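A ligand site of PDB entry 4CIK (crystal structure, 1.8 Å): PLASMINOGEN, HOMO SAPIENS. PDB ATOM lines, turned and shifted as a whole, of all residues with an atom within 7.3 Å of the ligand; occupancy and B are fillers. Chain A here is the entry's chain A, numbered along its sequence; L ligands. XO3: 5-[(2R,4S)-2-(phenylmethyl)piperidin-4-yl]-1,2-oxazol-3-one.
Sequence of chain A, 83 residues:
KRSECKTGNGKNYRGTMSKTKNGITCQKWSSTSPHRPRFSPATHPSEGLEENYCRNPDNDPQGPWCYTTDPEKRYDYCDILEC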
ATOM      1  N   ARG A  36      14.776  10.439 -16.211  1.00  0.00           N
ATOM      2  CA  ARG A  36      14.956  11.858 -15.922  1.00  0.00           C
ATOM      3  C   ARG A  36      13.959  12.656 -16.775  1.00  0.00           C
ATOM      4  O   ARG A  36      13.965  12.596 -17.994  1.00  0.00           O
ATOM      5  CB  ARG A  36      16.383  12.295 -16.168  1.00  0.00           C
ATOM      6  CG  ARG A  36      16.534  13.800 -16.003  1.00  0.00           C
ATOM      7  CD  ARG A  36      17.977  14.121 -15.777  1.00  0.00           C
ATOM      8  NE  ARG A  36      18.696  14.041 -17.033  1.00  0.00           N
ATOM      9  CZ  ARG A  36      18.592  14.927 -18.007  1.00  0.00           C
ATOM     10  NH1 ARG A  36      17.776  15.965 -17.875  1.00  0.00           N
ATOM     11  NH2 ARG A  36      19.318  14.802 -19.117  1.00  0.00           N
ATOM     12  N   PRO A  37      13.036  13.376 -16.144  1.00  0.00           N
ATOM     13  CA  PRO A  37      12.009  14.051 -16.953  1.00  0.00           C
ATOM     14  C   PRO A  37      12.451  15.263 -17.768  1.00  0.00           C
ATOM     15  O   PRO A  37      13.441  15.918 -17.453  1.00  0.00           O
ATOM     16  CB  PRO A  37      11.044  14.616 -15.892  1.00  0.00           C
ATOM     17  CG  PRO A  37      11.284  13.858 -14.665  1.00  0.00           C
ATOM     18  CD  PRO A  37      12.669  13.278 -14.717  1.00  0.00           C
ATOM     19  N   ARG A  38      11.630  15.569 -18.777  1.00  0.00           N
ATOM     20  CA  ARG A  38      11.766  16.796 -19.587  1.00  0.00           C
ATOM     21  C   ARG A  38      10.748  17.781 -18.991  1.00  0.00           C
ATOM     22  O   ARG A  38      10.865  19.012 -19.146  1.00  0.00           O
ATOM     23  CB  ARG A  38      11.404  16.520 -21.049  1.00  0.00           C
ATOM     24  CG  ARG A  38      12.541  15.972 -21.911  1.00  0.00           C
ATOM     25  CD  ARG A  38      12.174  16.044 -23.413  1.00  0.00           C
ATOM     26  NE  ARG A  38      10.900  15.392 -23.687  1.00  0.00           N
ATOM     27  CZ  ARG A  38       9.927  15.909 -24.438  1.00  0.00           C
ATOM     28  NH1 ARG A  38      10.072  17.101 -25.033  1.00  0.00           N
ATOM     29  NH2 ARG A  38       8.806  15.227 -24.587  1.00  0.00           N
ATOM     30  N   PHE A  39       9.747  17.237 -18.303  1.00  0.00           N
ATOM     31  CA  PHE A  39       8.677  18.002 -17.636  1.00  0.00           C
ATOM     32  C   PHE A  39       8.639  17.608 -16.173  1.00  0.00           C
ATOM     33  O   PHE A  39       8.429  16.441 -15.842  1.00  0.00           O
ATOM     34  CB  PHE A  39       7.319  17.729 -18.276  1.00  0.00           C
ATOM     35  CG  PHE A  39       7.221  18.153 -19.709  1.00  0.00           C
ATOM     36  CD1 PHE A  39       6.804  19.426 -20.045  1.00  0.00           C
ATOM     37  CD2 PHE A  39       7.524  17.254 -20.722  1.00  0.00           C
ATOM     38  CE1 PHE A  39       6.750  19.825 -21.407  1.00  0.00           C
ATOM     39  CE2 PHE A  39       7.466  17.625 -22.055  1.00  0.00           C
ATOM     40  CZ  PHE A  39       7.099  18.914 -22.402  1.00  0.00           C
ATOM     41  N   ARG A  55      -0.624  13.256 -16.438  1.00  0.00           N
ATOM     42  CA  ARG A  55      -0.832  14.642 -16.908  1.00  0.00           C
ATOM     43  C   ARG A  55      -0.460  14.703 -18.395  1.00  0.00           C
ATOM     44  O   ARG A  55       0.077  13.744 -18.980  1.00  0.00           O
ATOM     45  CB  ARG A  55       0.062  15.645 -16.125  1.00  0.00           C
ATOM     46  CG  ARG A  55      -0.246  15.775 -14.626  1.00  0.00           C
ATOM     47  CD  ARG A  55      -1.557  16.561 -14.426  1.00  0.00           C
ATOM     48  NE  ARG A  55      -1.982  16.646 -13.030  1.00  0.00           N
ATOM     49  CZ  ARG A  55      -2.835  15.814 -12.430  1.00  0.00           C
ATOM     50  NH1 ARG A  55      -3.329  14.769 -13.083  1.00  0.00           N
ATOM     51  NH2 ARG A  55      -3.184  16.017 -11.167  1.00  0.00           N
ATOM     52  N   ASN A  56      -0.689  15.881 -18.974  1.00  0.00           N
ATOM     53  CA  ASN A  56      -0.353  16.094 -20.382  1.00  0.00           C
ATOM     54  C   ASN A  56       0.402  17.426 -20.588  1.00  0.00           C
ATOM     55  O   ASN A  56      -0.123  18.336 -21.201  1.00  0.00           O
ATOM     56  CB  ASN A  56      -1.624  16.022 -21.234  1.00  0.00           C
ATOM     57  CG  ASN A  56      -1.317  15.801 -22.683  1.00  0.00           C
ATOM     58  OD1 ASN A  56      -0.155  15.677 -23.003  1.00  0.00           O
ATOM     59  ND2 ASN A  56      -2.321  15.532 -23.500  1.00  0.00           N
ATOM     60  N   PRO A  57       1.606  17.573 -19.992  1.00  0.00           N
ATOM     61  CA  PRO A  57       2.280  18.890 -20.120  1.00  0.00           C
ATOM     62  C   PRO A  57       2.759  19.209 -21.551  1.00  0.00           C
ATOM     63  O   PRO A  57       3.006  20.372 -21.899  1.00  0.00           O
ATOM     64  CB  PRO A  57       3.472  18.767 -19.150  1.00  0.00           C
ATOM     65  CG  PRO A  57       3.723  17.272 -19.027  1.00  0.00           C
ATOM     66  CD  PRO A  57       2.324  16.680 -19.049  1.00  0.00           C
ATOM     67  N   ASP A  58       2.765  18.190 -22.386  1.00  0.00           N
ATOM     68  CA  ASP A  58       3.214  18.361 -23.776  1.00  0.00           C
ATOM     69  C   ASP A  58       2.096  18.328 -24.841  1.00  0.00           C
ATOM     70  O   ASP A  58       2.362  18.205 -26.037  1.00  0.00           O
ATOM     71  CB  ASP A  58       4.364  17.386 -24.101  1.00  0.00           C
ATOM     72  CG  ASP A  58       3.909  15.943 -24.241  1.00  0.00           C
ATOM     73  OD1 ASP A  58       2.805  15.596 -23.724  1.00  0.00           O
ATOM     74  OD2 ASP A  58       4.634  15.180 -24.911  1.00  0.00           O
ATOM     75  N   ASN A  59       0.841  18.434 -24.400  1.00  0.00           N
ATOM     76  CA  ASN A  59      -0.286  18.509 -25.333  1.00  0.00           C
ATOM     77  C   ASN A  59      -0.375  17.325 -26.295  1.00  0.00           C
ATOM     78  O   ASN A  59      -0.781  17.492 -27.446  1.00  0.00           O
ATOM     79  CB  ASN A  59      -0.182  19.822 -26.119  1.00  0.00           C
ATOM     80  CG  ASN A  59      -1.517  20.276 -26.697  1.00  0.00           C
ATOM     81  OD1 ASN A  59      -2.581  19.889 -26.233  1.00  0.00           O
ATOM     82  ND2 ASN A  59      -1.451  21.154 -27.689  1.00  0.00           N
ATOM     83  N   ASP A  60      -0.007  16.118 -25.830  1.00  0.00           N
ATOM     84  CA  ASP A  60      -0.034  14.922 -26.657  1.00  0.00           C
ATOM     85  C   ASP A  60      -1.494  14.697 -27.072  1.00  0.00           C
ATOM     86  O   ASP A  60      -2.394  14.632 -26.229  1.00  0.00           O
ATOM     87  CB  ASP A  60       0.451  13.704 -25.842  1.00  0.00           C
ATOM     88  CG  ASP A  60       0.729  12.469 -26.715  1.00  0.00           C
ATOM     89  OD1 ASP A  60      -0.055  12.203 -27.638  1.00  0.00           O
ATOM     90  OD2 ASP A  60       1.724  11.750 -26.467  1.00  0.00           O
ATOM     91  N   PRO A  61      -1.739  14.519 -28.370  1.00  0.00           N
ATOM     92  CA  PRO A  61      -3.114  14.254 -28.787  1.00  0.00           C
ATOM     93  C   PRO A  61      -3.624  12.925 -28.220  1.00  0.00           C
ATOM     94  O   PRO A  61      -4.819  12.662 -28.233  1.00  0.00           O
ATOM     95  CB  PRO A  61      -3.002  14.128 -30.305  1.00  0.00           C
ATOM     96  CG  PRO A  61      -1.762  14.915 -30.670  1.00  0.00           C
ATOM     97  CD  PRO A  61      -0.815  14.706 -29.509  1.00  0.00           C
ATOM     98  N   GLN A  62      -2.717  12.077 -27.774  1.00  0.00           N
ATOM     99  CA  GLN A  62      -3.107  10.777 -27.215  1.00  0.00           C
ATOM    100  C   GLN A  62      -3.574  10.890 -25.775  1.00  0.00           C
ATOM    101  O   GLN A  62      -4.046   9.898 -25.206  1.00  0.00           O
ATOM    102  CB  GLN A  62      -1.957   9.793 -27.310  1.00  0.00           C
ATOM    103  CG  GLN A  62      -1.432   9.640 -28.709  1.00  0.00           C
ATOM    104  CD  GLN A  62      -2.153   8.561 -29.442  1.00  0.00           C
ATOM    105  OE1 GLN A  62      -2.019   7.382 -29.116  1.00  0.00           O
ATOM    106  NE2 GLN A  62      -3.009   8.959 -30.387  1.00  0.00           N
ATOM    107  N   GLY A  63      -3.448  12.093 -25.212  1.00  0.00           N
ATOM    108  CA  GLY A  63      -3.898  12.424 -23.869  1.00  0.00           C
ATOM    109  C   GLY A  63      -2.887  12.270 -22.750  1.00  0.00           C
ATOM    110  O   GLY A  63      -1.710  12.105 -22.981  1.00  0.00           O
ATOM    111  N   PRO A  64      -3.367  12.335 -21.496  1.00  0.00           N
ATOM    112  CA  PRO A  64      -2.476  12.248 -20.343  1.00  0.00           C
ATOM    113  C   PRO A  64      -1.656  10.979 -20.282  1.00  0.00           C
ATOM    114  O   PRO A  64      -2.094   9.875 -20.673  1.00  0.00           O
ATOM    115  CB  PRO A  64      -3.423  12.335 -19.139  1.00  0.00           C
ATOM    116  CG  PRO A  64      -4.635  13.043 -19.683  1.00  0.00           C
ATOM    117  CD  PRO A  64      -4.759  12.543 -21.101  1.00  0.00           C
ATOM    118  N   TRP A  65      -0.487  11.136 -19.677  1.00  0.00           N
ATOM    119  CA  TRP A  65       0.463  10.059 -19.547  1.00  0.00           C
ATOM    120  C   TRP A  65       1.333  10.311 -18.321  1.00  0.00           C
ATOM    121  O   TRP A  65       1.147  11.296 -17.601  1.00  0.00           O
ATOM    122  CB  TRP A  65       1.343  10.085 -20.794  1.00  0.00           C
ATOM    123  CG  TRP A  65       1.917  11.430 -21.071  1.00  0.00           C
ATOM    124  CD1 TRP A  65       1.374  12.394 -21.838  1.00  0.00           C
ATOM    125  CD2 TRP A  65       3.164  11.973 -20.567  1.00  0.00           C
ATOM    126  NE1 TRP A  65       2.180  13.501 -21.869  1.00  0.00           N
ATOM    127  CE2 TRP A  65       3.323  13.251 -21.149  1.00  0.00           C
ATOM    128  CE3 TRP A  65       4.187  11.472 -19.766  1.00  0.00           C
ATOM    129  CZ2 TRP A  65       4.436  14.065 -20.889  1.00  0.00           C
ATOM    130  CZ3 TRP A  65       5.330  12.267 -19.559  1.00  0.00           C
ATOM    131  CH2 TRP A  65       5.430  13.555 -20.115  1.00  0.00           C
ATOM    132  N   CYS A  66       2.325   9.450 -18.120  1.00  0.00           N
ATOM    133  CA  CYS A  66       3.256   9.663 -17.002  1.00  0.00           C
ATOM    134  C   CYS A  66       4.577   8.982 -17.239  1.00  0.00           C
ATOM    135  O   CYS A  66       4.628   8.021 -17.947  1.00  0.00           O
ATOM    136  CB  CYS A  66       2.666   9.147 -15.687  1.00  0.00           C
ATOM    137  SG  CYS A  66       2.497   7.358 -15.602  1.00  0.00           S
ATOM    138  N   TYR A  67       5.651   9.456 -16.611  1.00  0.00           N
ATOM    139  CA  TYR A  67       6.893   8.687 -16.695  1.00  0.00           C
ATOM    140  C   TYR A  67       6.588   7.462 -15.823  1.00  0.00           C
ATOM    141  O   TYR A  67       5.901   7.608 -14.812  1.00  0.00           O
ATOM    142  CB  TYR A  67       8.090   9.499 -16.162  1.00  0.00           C
ATOM    143  CG  TYR A  67       8.455  10.667 -17.043  1.00  0.00           C
ATOM    144  CD1 TYR A  67       8.982  10.470 -18.310  1.00  0.00           C
ATOM    145  CD2 TYR A  67       8.153  11.979 -16.659  1.00  0.00           C
ATOM    146  CE1 TYR A  67       9.325  11.535 -19.117  1.00  0.00           C
ATOM    147  CE2 TYR A  67       8.419  13.041 -17.504  1.00  0.00           C
ATOM    148  CZ  TYR A  67       9.051  12.827 -18.701  1.00  0.00           C
ATOM    149  OH  TYR A  67       9.356  13.867 -19.549  1.00  0.00           O
ATOM    150  N   ARG A  74       9.947   4.401 -20.683  1.00  0.00           N
ATOM    151  CA  ARG A  74      10.038   5.775 -20.177  1.00  0.00           C
ATOM    152  C   ARG A  74       8.693   6.395 -19.814  1.00  0.00           C
ATOM    153  O   ARG A  74       8.557   7.022 -18.773  1.00  0.00           O
ATOM    154  CB  ARG A  74      10.750   6.673 -21.173  1.00  0.00           C
ATOM    155  CG  ARG A  74      10.954   8.065 -20.658  1.00  0.00           C
ATOM    156  CD  ARG A  74      11.989   8.714 -21.526  1.00  0.00           C
ATOM    157  NE  ARG A  74      11.928  10.156 -21.380  1.00  0.00           N
ATOM    158  CZ  ARG A  74      12.662  10.843 -20.523  1.00  0.00           C
ATOM    159  NH1 ARG A  74      13.565  10.237 -19.754  1.00  0.00           N
ATOM    160  NH2 ARG A  74      12.480  12.138 -20.438  1.00  0.00           N
ATOM    161  N   TYR A  75       7.744   6.292 -20.727  1.00  0.00           N
ATOM    162  CA  TYR A  75       6.444   6.883 -20.494  1.00  0.00           C
ATOM    163  C   TYR A  75       5.362   5.975 -21.033  1.00  0.00           C
ATOM    164  O   TYR A  75       5.602   5.084 -21.871  1.00  0.00           O
ATOM    165  CB  TYR A  75       6.330   8.271 -21.195  1.00  0.00           C
ATOM    166  CG  TYR A  75       6.253   8.177 -22.723  1.00  0.00           C
ATOM    167  CD1 TYR A  75       7.405   8.168 -23.503  1.00  0.00           C
ATOM    168  CD2 TYR A  75       5.010   8.160 -23.380  1.00  0.00           C
ATOM    169  CE1 TYR A  75       7.326   8.067 -24.899  1.00  0.00           C
ATOM    170  CE2 TYR A  75       4.926   8.084 -24.749  1.00  0.00           C
ATOM    171  CZ  TYR A  75       6.096   8.040 -25.509  1.00  0.00           C
ATOM    172  OH  TYR A  75       6.020   7.962 -26.889  1.00  0.00           O
ATOM    173  N   ASP A  76       4.148   6.255 -20.611  1.00  0.00           N
ATOM    174  CA  ASP A  76       3.003   5.554 -21.152  1.00  0.00           C
ATOM    175  C   ASP A  76       1.746   6.295 -20.818  1.00  0.00           C
ATOM    176  O   ASP A  76       1.662   7.004 -19.843  1.00  0.00           O
ATOM    177  CB  ASP A  76       2.947   4.130 -20.638  1.00  0.00           C
ATOM    178  CG  ASP A  76       2.049   3.248 -21.489  1.00  0.00           C
ATOM    179  OD1 ASP A  76       1.671   3.683 -22.589  1.00  0.00           O
ATOM    180  OD2 ASP A  76       1.691   2.137 -21.028  1.00  0.00           O
ATOM    181  N   TYR A  77       0.722   6.042 -21.618  1.00  0.00           N
ATOM    182  CA  TYR A  77      -0.583   6.623 -21.369  1.00  0.00           C
ATOM    183  C   TYR A  77      -1.377   5.937 -20.267  1.00  0.00           C
ATOM    184  O   TYR A  77      -1.160   4.765 -19.936  1.00  0.00           O
ATOM    185  CB  TYR A  77      -1.366   6.660 -22.672  1.00  0.00           C
ATOM    186  CG  TYR A  77      -0.587   7.355 -23.759  1.00  0.00           C
ATOM    187  CD1 TYR A  77      -0.543   8.742 -23.818  1.00  0.00           C
ATOM    188  CD2 TYR A  77       0.159   6.632 -24.695  1.00  0.00           C
ATOM    189  CE1 TYR A  77       0.230   9.396 -24.761  1.00  0.00           C
ATOM    190  CE2 TYR A  77       0.941   7.271 -25.620  1.00  0.00           C
ATOM    191  CZ  TYR A  77       0.949   8.667 -25.671  1.00  0.00           C
ATOM    192  OH  TYR A  77       1.696   9.323 -26.633  1.00  0.00           O
HETATM  193  C1  XO3 L   1       5.467  11.934 -23.507  1.00  0.00           C
HETATM  194  C2  XO3 L   1       4.127  11.579 -24.173  1.00  0.00           C
HETATM  195  N3  XO3 L   1       4.091  12.414 -25.397  1.00  0.00           N
HETATM  196  C4  XO3 L   1       5.122  11.950 -26.359  1.00  0.00           C
HETATM  197  C5  XO3 L   1       6.517  12.285 -25.764  1.00  0.00           C
HETATM  198  C6  XO3 L   1       6.603  11.514 -24.445  1.00  0.00           C
HETATM  199  C7  XO3 L   1       7.946  11.815 -23.864  1.00  0.00           C
HETATM  200  O8  XO3 L   1       9.109  11.334 -24.313  1.00  0.00           O
HETATM  201  N9  XO3 L   1      10.048  11.735 -23.637  1.00  0.00           N
HETATM  202  C10 XO3 L   1       9.609  12.587 -22.697  1.00  0.00           C
HETATM  203  C11 XO3 L   1       8.195  12.658 -22.849  1.00  0.00           C
HETATM  204  O12 XO3 L   1      10.257  13.183 -21.877  1.00  0.00           O
HETATM  205  C13 XO3 L   1       4.986  12.770 -27.636  1.00  0.00           C
HETATM  206  C14 XO3 L   1       5.798  12.156 -28.763  1.00  0.00           C
HETATM  207  C15 XO3 L   1       6.762  12.918 -29.402  1.00  0.00           C
HETATM  208  C16 XO3 L   1       7.479  12.388 -30.465  1.00  0.00           C
HETATM  209  C17 XO3 L   1       7.256  11.084 -30.876  1.00  0.00           C
HETATM  210  C18 XO3 L   1       6.280  10.332 -30.247  1.00  0.00           C
HETATM  211  C19 XO3 L   1       5.556  10.857 -29.189  1.00  0.00           C
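The side-chain carboxylate (OD2) of Asp 60 lies within salt-bridge range of a nitrogen (N3) of the ligand (2.7 Å). An oxygen (O12) of the ligand is in hydrogen-bond range of the side-chain hydroxyl (OH) of Tyr 67 (2.6 Å). NH2 of Arg 74 is in hydrogen-bond range of O12 of the ligand (2.8 Å). An oxygen (O12) of the ligand lies within hydrogen-bond range of the guanidinium group (NE) of Arg 38, at 2.9 Å. The side-chain carboxylate (OD2) of Asp 58 lies within salt-bridge range of a nitrogen (N3) of the ligand, at 2.9 Å.
OD1 of Asn 56 sits close to OD1 of Asp 58 (3.0 Å). The backbone NH (N) of Asp 60 lies within hydrogen-bond range of the side-chain amide oxygen (OD1) of Asn 56 (2.9 Å). The side-chain carboxylate of Asp 58 sits at hydrogen-bond distance from the indole nitrogen of Trp 65 (2.9 Å). OH of Tyr 77 sits at hydrogen-bond distance from OD2 of Asp 60. The backbone NH (N) of Trp 65 lies within hydrogen-bond range of the backbone carbonyl oxygen (O) of Arg 55, 2.8 Å away. The indole nitrogen (NE1) of Trp 65 sits at hydrogen-bond distance from the side-chain amide oxygen (OD1) of Asn 56 (3.4 Å). The backbone carbonyl oxygen of Arg 36 lies within hydrogen-bond range of the guanidinium group of Arg 74 (2.9 Å). N of Gln 62 is in hydrogen-bond range of OD1 of Asp 60 (2.7 Å).
Merely in contact with the ligand: Trp 65 and Tyr 75. Within 4 Å of the ligand: Arg 38, Asp 58, Asp 60, Trp 65, Tyr 67, Arg 74 and Tyr 75. The nearest printed residue that does not touch the ligand is Tyr 77 (4.1 Å).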
